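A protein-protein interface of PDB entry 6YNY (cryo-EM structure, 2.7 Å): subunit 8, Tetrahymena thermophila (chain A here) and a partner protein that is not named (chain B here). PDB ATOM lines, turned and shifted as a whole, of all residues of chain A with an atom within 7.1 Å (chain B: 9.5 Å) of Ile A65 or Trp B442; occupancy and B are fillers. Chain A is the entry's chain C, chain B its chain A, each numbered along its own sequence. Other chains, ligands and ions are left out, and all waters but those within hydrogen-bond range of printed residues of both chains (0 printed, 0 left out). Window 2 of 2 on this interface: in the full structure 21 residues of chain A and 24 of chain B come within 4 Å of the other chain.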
ATOM      1  N   SER A  61     -18.243  20.825 -15.420  1.00  0.00           N
ATOM      2  CA  SER A  61     -19.146  20.247 -16.400  1.00  0.00           C
ATOM      3  C   SER A  61     -20.024  19.210 -15.718  1.00  0.00           C
ATOM      4  O   SER A  61     -19.627  18.592 -14.729  1.00  0.00           O
ATOM      5  CB  SER A  61     -18.378  19.609 -17.560  1.00  0.00           C
ATOM      6  OG  SER A  61     -19.250  19.232 -18.606  1.00  0.00           O
ATOM      7  N   GLN A  62     -21.225  19.022 -16.264  1.00  0.00           N
ATOM      8  CA  GLN A  62     -22.195  18.119 -15.658  1.00  0.00           C
ATOM      9  C   GLN A  62     -21.873  16.652 -15.890  1.00  0.00           C
ATOM     10  O   GLN A  62     -22.368  15.803 -15.142  1.00  0.00           O
ATOM     11  CB  GLN A  62     -23.598  18.423 -16.188  1.00  0.00           C
ATOM     12  CG  GLN A  62     -24.363  19.423 -15.347  1.00  0.00           C
ATOM     13  CD  GLN A  62     -24.613  18.915 -13.938  1.00  0.00           C
ATOM     14  OE1 GLN A  62     -25.276  17.896 -13.743  1.00  0.00           O
ATOM     15  NE2 GLN A  62     -24.066  19.611 -12.953  1.00  0.00           N
ATOM     16  N   GLU A  63     -21.069  16.330 -16.895  1.00  0.00           N
ATOM     17  CA  GLU A  63     -20.664  14.951 -17.127  1.00  0.00           C
ATOM     18  C   GLU A  63     -19.485  14.531 -16.259  1.00  0.00           C
ATOM     19  O   GLU A  63     -18.947  13.438 -16.463  1.00  0.00           O
ATOM     20  CB  GLU A  63     -20.323  14.735 -18.605  1.00  0.00           C
ATOM     21  CG  GLU A  63     -19.405  15.777 -19.204  1.00  0.00           C
ATOM     22  CD  GLU A  63     -20.163  16.870 -19.925  1.00  0.00           C
ATOM     23  OE1 GLU A  63     -20.072  16.937 -21.168  1.00  0.00           O
ATOM     24  OE2 GLU A  63     -20.854  17.660 -19.249  1.00  0.00           O
ATOM     25  N   PHE A  64     -19.077  15.362 -15.304  1.00  0.00           N
ATOM     26  CA  PHE A  64     -17.998  15.025 -14.389  1.00  0.00           C
ATOM     27  C   PHE A  64     -18.372  15.472 -12.986  1.00  0.00           C
ATOM     28  O   PHE A  64     -19.255  16.310 -12.791  1.00  0.00           O
ATOM     29  CB  PHE A  64     -16.671  15.669 -14.806  1.00  0.00           C
ATOM     30  CG  PHE A  64     -16.249  15.332 -16.199  1.00  0.00           C
ATOM     31  CD1 PHE A  64     -15.776  14.073 -16.507  1.00  0.00           C
ATOM     32  CD2 PHE A  64     -16.325  16.276 -17.203  1.00  0.00           C
ATOM     33  CE1 PHE A  64     -15.392  13.763 -17.786  1.00  0.00           C
ATOM     34  CE2 PHE A  64     -15.942  15.971 -18.482  1.00  0.00           C
ATOM     35  CZ  PHE A  64     -15.474  14.713 -18.777  1.00  0.00           C
ATOM     36  N   ILE A  65     -17.687  14.897 -12.008  1.00  0.00           N
ATOM     37  CA  ILE A  65     -17.904  15.222 -10.605  1.00  0.00           C
ATOM     38  C   ILE A  65     -16.965  16.350 -10.207  1.00  0.00           C
ATOM     39  O   ILE A  65     -15.753  16.273 -10.439  1.00  0.00           O
ATOM     40  CB  ILE A  65     -17.680  13.990  -9.713  1.00  0.00           C
ATOM     41  CG1 ILE A  65     -18.642  12.868 -10.093  1.00  0.00           C
ATOM     42  CG2 ILE A  65     -17.848  14.360  -8.253  1.00  0.00           C
ATOM     43  CD1 ILE A  65     -18.353  11.569  -9.400  1.00  0.00           C
ATOM     44  N   ARG A  66     -17.521  17.396  -9.605  1.00  0.00           N
ATOM     45  CA  ARG A  66     -16.723  18.468  -9.030  1.00  0.00           C
ATOM     46  C   ARG A  66     -16.475  18.144  -7.564  1.00  0.00           C
ATOM     47  O   ARG A  66     -17.420  18.048  -6.775  1.00  0.00           O
ATOM     48  CB  ARG A  66     -17.420  19.820  -9.174  1.00  0.00           C
ATOM     49  CG  ARG A  66     -16.618  20.974  -8.603  1.00  0.00           C
ATOM     50  CD  ARG A  66     -17.374  22.280  -8.648  1.00  0.00           C
ATOM     51  NE  ARG A  66     -16.739  23.289  -7.808  1.00  0.00           N
ATOM     52  CZ  ARG A  66     -17.306  24.435  -7.451  1.00  0.00           C
ATOM     53  NH1 ARG A  66     -18.530  24.730  -7.855  1.00  0.00           N
ATOM     54  NH2 ARG A  66     -16.649  25.285  -6.681  1.00  0.00           N
ATOM     55  N   PHE A  67     -15.209  17.969  -7.205  1.00  0.00           N
ATOM     56  CA  PHE A  67     -14.842  17.603  -5.848  1.00  0.00           C
ATOM     57  C   PHE A  67     -14.526  18.843  -5.028  1.00  0.00           C
ATOM     58  O   PHE A  67     -13.942  19.807  -5.527  1.00  0.00           O
ATOM     59  CB  PHE A  67     -13.647  16.654  -5.851  1.00  0.00           C
ATOM     60  CG  PHE A  67     -13.943  15.318  -6.457  1.00  0.00           C
ATOM     61  CD1 PHE A  67     -14.568  14.335  -5.718  1.00  0.00           C
ATOM     62  CD2 PHE A  67     -13.600  15.046  -7.765  1.00  0.00           C
ATOM     63  CE1 PHE A  67     -14.843  13.110  -6.271  1.00  0.00           C
ATOM     64  CE2 PHE A  67     -13.875  13.820  -8.321  1.00  0.00           C
ATOM     65  CZ  PHE A  67     -14.498  12.853  -7.572  1.00  0.00           C
ATOM     66  N   ARG A  68     -14.922  18.803  -3.762  1.00  0.00           N
ATOM     67  CA  ARG A  68     -14.784  19.952  -2.884  1.00  0.00           C
ATOM     68  C   ARG A  68     -13.332  20.133  -2.457  1.00  0.00           C
ATOM     69  O   ARG A  68     -12.615  19.161  -2.209  1.00  0.00           O
ATOM     70  CB  ARG A  68     -15.680  19.770  -1.665  1.00  0.00           C
ATOM     71  CG  ARG A  68     -15.928  21.017  -0.865  1.00  0.00           C
ATOM     72  CD  ARG A  68     -16.893  20.745   0.264  1.00  0.00           C
ATOM     73  NE  ARG A  68     -18.213  20.359  -0.220  1.00  0.00           N
ATOM     74  CZ  ARG A  68     -19.210  21.205  -0.454  1.00  0.00           C
ATOM     75  NH1 ARG A  68     -19.056  22.503  -0.251  1.00  0.00           N
ATOM     76  NH2 ARG A  68     -20.371  20.748  -0.893  1.00  0.00           N
ATOM     77  N   ARG B 431      -6.679   4.752  -8.170  1.00  0.00           N
ATOM     78  CA  ARG B 431      -7.765   5.321  -8.957  1.00  0.00           C
ATOM     79  C   ARG B 431      -8.818   4.279  -9.293  1.00  0.00           C
ATOM     80  O   ARG B 431     -10.010   4.600  -9.364  1.00  0.00           O
ATOM     81  CB  ARG B 431      -7.208   5.940 -10.235  1.00  0.00           C
ATOM     82  CG  ARG B 431      -6.303   7.123  -9.998  1.00  0.00           C
ATOM     83  CD  ARG B 431      -5.566   7.529 -11.251  1.00  0.00           C
ATOM     84  NE  ARG B 431      -6.469   7.989 -12.300  1.00  0.00           N
ATOM     85  CZ  ARG B 431      -7.031   9.191 -12.330  1.00  0.00           C
ATOM     86  NH1 ARG B 431      -7.832   9.518 -13.327  1.00  0.00           N
ATOM     87  NH2 ARG B 431      -6.803  10.063 -11.363  1.00  0.00           N
ATOM     88  N   GLU B 432      -8.404   3.031  -9.505  1.00  0.00           N
ATOM     89  CA  GLU B 432      -9.365   1.964  -9.754  1.00  0.00           C
ATOM     90  C   GLU B 432     -10.198   1.681  -8.511  1.00  0.00           C
ATOM     91  O   GLU B 432     -11.428   1.590  -8.582  1.00  0.00           O
ATOM     92  CB  GLU B 432      -8.634   0.705 -10.210  1.00  0.00           C
ATOM     93  CG  GLU B 432      -7.893   0.868 -11.521  1.00  0.00           C
ATOM     94  CD  GLU B 432      -7.037  -0.335 -11.863  1.00  0.00           C
ATOM     95  OE1 GLU B 432      -6.968  -1.272 -11.039  1.00  0.00           O
ATOM     96  OE2 GLU B 432      -6.431  -0.344 -12.956  1.00  0.00           O
ATOM     97  N   ARG B 434     -10.591   3.702  -5.954  1.00  0.00           N
ATOM     98  CA  ARG B 434     -11.343   4.908  -5.639  1.00  0.00           C
ATOM     99  C   ARG B 434     -12.555   5.062  -6.546  1.00  0.00           C
ATOM    100  O   ARG B 434     -13.565   5.643  -6.136  1.00  0.00           O
ATOM    101  CB  ARG B 434     -10.425   6.124  -5.750  1.00  0.00           C
ATOM    102  CG  ARG B 434     -11.085   7.462  -5.495  1.00  0.00           C
ATOM    103  CD  ARG B 434     -11.539   7.622  -4.064  1.00  0.00           C
ATOM    104  NE  ARG B 434     -12.176   8.917  -3.861  1.00  0.00           N
ATOM    105  CZ  ARG B 434     -12.701   9.324  -2.713  1.00  0.00           C
ATOM    106  NH1 ARG B 434     -12.671   8.535  -1.648  1.00  0.00           N
ATOM    107  NH2 ARG B 434     -13.256  10.522  -2.634  1.00  0.00           N
ATOM    108  N   LYS B 435     -12.477   4.552  -7.776  1.00  0.00           N
ATOM    109  CA  LYS B 435     -13.617   4.637  -8.679  1.00  0.00           C
ATOM    110  C   LYS B 435     -14.726   3.678  -8.273  1.00  0.00           C
ATOM    111  O   LYS B 435     -15.903   3.950  -8.531  1.00  0.00           O
ATOM    112  CB  LYS B 435     -13.175   4.356 -10.114  1.00  0.00           C
ATOM    113  CG  LYS B 435     -14.276   4.553 -11.132  1.00  0.00           C
ATOM    114  CD  LYS B 435     -13.785   4.316 -12.545  1.00  0.00           C
ATOM    115  CE  LYS B 435     -14.932   4.380 -13.544  1.00  0.00           C
ATOM    116  NZ  LYS B 435     -15.677   5.668 -13.471  1.00  0.00           N
ATOM    117  N   LYS B 436     -14.376   2.551  -7.652  1.00  0.00           N
ATOM    118  CA  LYS B 436     -15.397   1.639  -7.155  1.00  0.00           C
ATOM    119  C   LYS B 436     -16.072   2.193  -5.910  1.00  0.00           C
ATOM    120  O   LYS B 436     -17.235   1.874  -5.641  1.00  0.00           O
ATOM    121  CB  LYS B 436     -14.782   0.275  -6.860  1.00  0.00           C
ATOM    122  CG  LYS B 436     -14.126  -0.375  -8.062  1.00  0.00           C
ATOM    123  CD  LYS B 436     -13.381  -1.646  -7.685  1.00  0.00           C
ATOM    124  CE  LYS B 436     -14.326  -2.746  -7.233  1.00  0.00           C
ATOM    125  NZ  LYS B 436     -15.277  -3.141  -8.307  1.00  0.00           N
ATOM    126  N   LYS B 437     -15.361   3.018  -5.144  1.00  0.00           N
ATOM    127  CA  LYS B 437     -15.958   3.647  -3.972  1.00  0.00           C
ATOM    128  C   LYS B 437     -16.986   4.699  -4.368  1.00  0.00           C
ATOM    129  O   LYS B 437     -17.909   4.982  -3.598  1.00  0.00           O
ATOM    130  CB  LYS B 437     -14.851   4.257  -3.111  1.00  0.00           C
ATOM    131  CG  LYS B 437     -15.317   4.924  -1.830  1.00  0.00           C
ATOM    132  CD  LYS B 437     -15.921   3.925  -0.863  1.00  0.00           C
ATOM    133  CE  LYS B 437     -16.348   4.593   0.429  1.00  0.00           C
ATOM    134  NZ  LYS B 437     -16.872   3.610   1.410  1.00  0.00           N
ATOM    135  N   LEU B 438     -16.847   5.282  -5.559  1.00  0.00           N
ATOM    136  CA  LEU B 438     -17.771   6.279  -6.080  1.00  0.00           C
ATOM    137  C   LEU B 438     -18.692   5.715  -7.155  1.00  0.00           C
ATOM    138  O   LEU B 438     -19.219   6.475  -7.974  1.00  0.00           O
ATOM    139  CB  LEU B 438     -16.992   7.468  -6.641  1.00  0.00           C
ATOM    140  CG  LEU B 438     -16.420   8.493  -5.663  1.00  0.00           C
ATOM    141  CD1 LEU B 438     -15.663   7.827  -4.542  1.00  0.00           C
ATOM    142  CD2 LEU B 438     -15.508   9.431  -6.422  1.00  0.00           C
ATOM    143  N   LYS B 439     -18.901   4.400  -7.168  1.00  0.00           N
ATOM    144  CA  LYS B 439     -19.694   3.789  -8.228  1.00  0.00           C
ATOM    145  C   LYS B 439     -21.143   4.253  -8.183  1.00  0.00           C
ATOM    146  O   LYS B 439     -21.778   4.437  -9.227  1.00  0.00           O
ATOM    147  CB  LYS B 439     -19.619   2.270  -8.111  1.00  0.00           C
ATOM    148  CG  LYS B 439     -20.307   1.520  -9.229  1.00  0.00           C
ATOM    149  CD  LYS B 439     -20.264   0.026  -8.988  1.00  0.00           C
ATOM    150  CE  LYS B 439     -20.920  -0.739 -10.120  1.00  0.00           C
ATOM    151  NZ  LYS B 439     -22.348  -0.364 -10.293  1.00  0.00           N
ATOM    152  N   GLU B 440     -21.686   4.448  -6.982  1.00  0.00           N
ATOM    153  CA  GLU B 440     -23.092   4.814  -6.863  1.00  0.00           C
ATOM    154  C   GLU B 440     -23.329   6.257  -7.282  1.00  0.00           C
ATOM    155  O   GLU B 440     -24.327   6.560  -7.943  1.00  0.00           O
ATOM    156  CB  GLU B 440     -23.572   4.591  -5.432  1.00  0.00           C
ATOM    157  CG  GLU B 440     -23.521   3.142  -4.979  1.00  0.00           C
ATOM    158  CD  GLU B 440     -22.118   2.682  -4.631  1.00  0.00           C
ATOM    159  OE1 GLU B 440     -21.185   3.510  -4.701  1.00  0.00           O
ATOM    160  OE2 GLU B 440     -21.947   1.492  -4.292  1.00  0.00           O
ATOM    161  N   LEU B 441     -22.423   7.160  -6.910  1.00  0.00           N
ATOM    162  CA  LEU B 441     -22.582   8.557  -7.293  1.00  0.00           C
ATOM    163  C   LEU B 441     -22.527   8.722  -8.805  1.00  0.00           C
ATOM    164  O   LEU B 441     -23.265   9.533  -9.375  1.00  0.00           O
ATOM    165  CB  LEU B 441     -21.510   9.405  -6.615  1.00  0.00           C
ATOM    166  CG  LEU B 441     -21.473  10.882  -7.008  1.00  0.00           C
ATOM    167  CD1 LEU B 441     -22.835  11.530  -6.856  1.00  0.00           C
ATOM    168  CD2 LEU B 441     -20.447  11.601  -6.170  1.00  0.00           C
ATOM    169  N   TRP B 442     -21.655   7.966  -9.473  1.00  0.00           N
ATOM    170  CA  TRP B 442     -21.638   7.995 -10.931  1.00  0.00           C
ATOM    171  C   TRP B 442     -22.936   7.451 -11.508  1.00  0.00           C
ATOM    172  O   TRP B 442     -23.418   7.937 -12.537  1.00  0.00           O
ATOM    173  CB  TRP B 442     -20.452   7.197 -11.462  1.00  0.00           C
ATOM    174  CG  TRP B 442     -19.160   7.930 -11.409  1.00  0.00           C
ATOM    175  CD1 TRP B 442     -18.111   7.684 -10.580  1.00  0.00           C
ATOM    176  CD2 TRP B 442     -18.775   9.039 -12.225  1.00  0.00           C
ATOM    177  NE1 TRP B 442     -17.094   8.568 -10.828  1.00  0.00           N
ATOM    178  CE2 TRP B 442     -17.478   9.413 -11.835  1.00  0.00           C
ATOM    179  CE3 TRP B 442     -19.403   9.753 -13.247  1.00  0.00           C
ATOM    180  CZ2 TRP B 442     -16.797  10.467 -12.429  1.00  0.00           C
ATOM    181  CZ3 TRP B 442     -18.726  10.798 -13.835  1.00  0.00           C
ATOM    182  CH2 TRP B 442     -17.435  11.146 -13.426  1.00  0.00           C
ATOM    183  N   ASN B 443     -23.518   6.440 -10.860  1.00  0.00           N
ATOM    184  CA  ASN B 443     -24.780   5.890 -11.339  1.00  0.00           C
ATOM    185  C   ASN B 443     -25.862   6.957 -11.390  1.00  0.00           C
ATOM    186  O   ASN B 443     -26.758   6.894 -12.238  1.00  0.00           O
ATOM    187  CB  ASN B 443     -25.210   4.729 -10.447  1.00  0.00           C
ATOM    188  CG  ASN B 443     -26.400   3.979 -11.001  1.00  0.00           C
ATOM    189  OD1 ASN B 443     -27.549   4.345 -10.760  1.00  0.00           O
ATOM    190  ND2 ASN B 443     -26.129   2.918 -11.748  1.00  0.00           N
ATOM    191  N   LEU B 444     -25.794   7.941 -10.500  1.00  0.00           N
ATOM    192  CA  LEU B 444     -26.709   9.073 -10.522  1.00  0.00           C
ATOM    193  C   LEU B 444     -26.349  10.094 -11.589  1.00  0.00           C
ATOM    194  O   LEU B 444     -27.031  11.119 -11.695  1.00  0.00           O
ATOM    195  CB  LEU B 444     -26.729   9.758  -9.158  1.00  0.00           C
ATOM    196  CG  LEU B 444     -26.968   8.865  -7.946  1.00  0.00           C
ATOM    197  CD1 LEU B 444     -26.868   9.679  -6.680  1.00  0.00           C
ATOM    198  CD2 LEU B 444     -28.313   8.190  -8.036  1.00  0.00           C
ATOM    199  N   LYS B 445     -25.301   9.844 -12.373  1.00  0.00           N
ATOM    200  CA  LYS B 445     -24.835  10.784 -13.389  1.00  0.00           C
ATOM    201  C   LYS B 445     -24.354  12.084 -12.760  1.00  0.00           C
ATOM    202  O   LYS B 445     -24.518  13.162 -13.335  1.00  0.00           O
ATOM    203  CB  LYS B 445     -25.921  11.058 -14.429  1.00  0.00           C
ATOM    204  CG  LYS B 445     -26.412   9.805 -15.122  1.00  0.00           C
ATOM    205  CD  LYS B 445     -27.430  10.126 -16.195  1.00  0.00           C
ATOM    206  CE  LYS B 445     -27.949   8.862 -16.844  1.00  0.00           C
ATOM    207  NZ  LYS B 445     -26.851   8.060 -17.454  1.00  0.00           N
ATOM    208  N   ASN B 446     -23.752  11.976 -11.579  1.00  0.00           N
ATOM    209  CA  ASN B 446     -23.221  13.118 -10.842  1.00  0.00           C
ATOM    210  C   ASN B 446     -24.164  14.315 -10.884  1.00  0.00           C
ATOM    211  O   ASN B 446     -24.624  14.789  -9.846  1.00  0.00           O
ATOM    212  CB  ASN B 446     -21.852  13.514 -11.391  1.00  0.00           C
ATOM    213  CG  ASN B 446     -21.939  14.209 -12.726  1.00  0.00           C
ATOM    214  OD1 ASN B 446     -21.897  13.570 -13.778  1.00  0.00           O
ATOM    215  ND2 ASN B 446     -22.065  15.529 -12.694  1.00  0.00           N
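Printed residues of chain A that touch a printed residue of chain B: Gln A62, Glu A63, Phe A64, Ile A65 and Phe A67. Hydrophobic or aromatic side chains of chain A within 4 Å of the printed part of chain B: Ile A65 and Phe A67. Of the 15 printed residues of chain B, 5 touch a printed residue of chain A. Hydrophobic or aromatic side chains of chain B within 4 Å of the printed part of chain A: Leu B438, Leu B441 and Trp B442.
The backbone carbonyl oxygen (O) of Leu B441 lies within hydrogen-bond range of the backbone NH (N) of Asn B446.
Lys B445 touches Gln A62 (O to O, 3.9 Å). Trp B442 touches Glu A63. OD1 of Asn B446 touches C of Glu A63, 3.6 Å away. CD2 of Leu B441 touches CD1 of Ile A65, 3.8 Å away. Ile A65 touches Trp B442 (CD1 to CE2, 3.4 Å). Asn B446 touches Ile A65 (CB to CG1, 3.5 Å). Leu B438 touches Phe A67 (CD2 to CE1, 3.7 Å).
ND2 of Asn B446 is in hydrogen-bond range of O of Gln A62. ND2 of Asn B446 lies within hydrogen-bond range of O of Phe A64 (2.9 Å).
Trp B442 touches two residues of chain A. Of the printed residues of chain B, Phe A67 touches Leu B438. Printed residues of chain A within 4 Å of Asn B446: Gln A62 (2.5 Å), Glu A63 (3.6 Å), Phe A64 (2.9 Å) and Ile A65 (3.5 Å). Lys B435 touches none of the printed residues of chain A. Lys B439 touches none of the printed residues of chain A.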
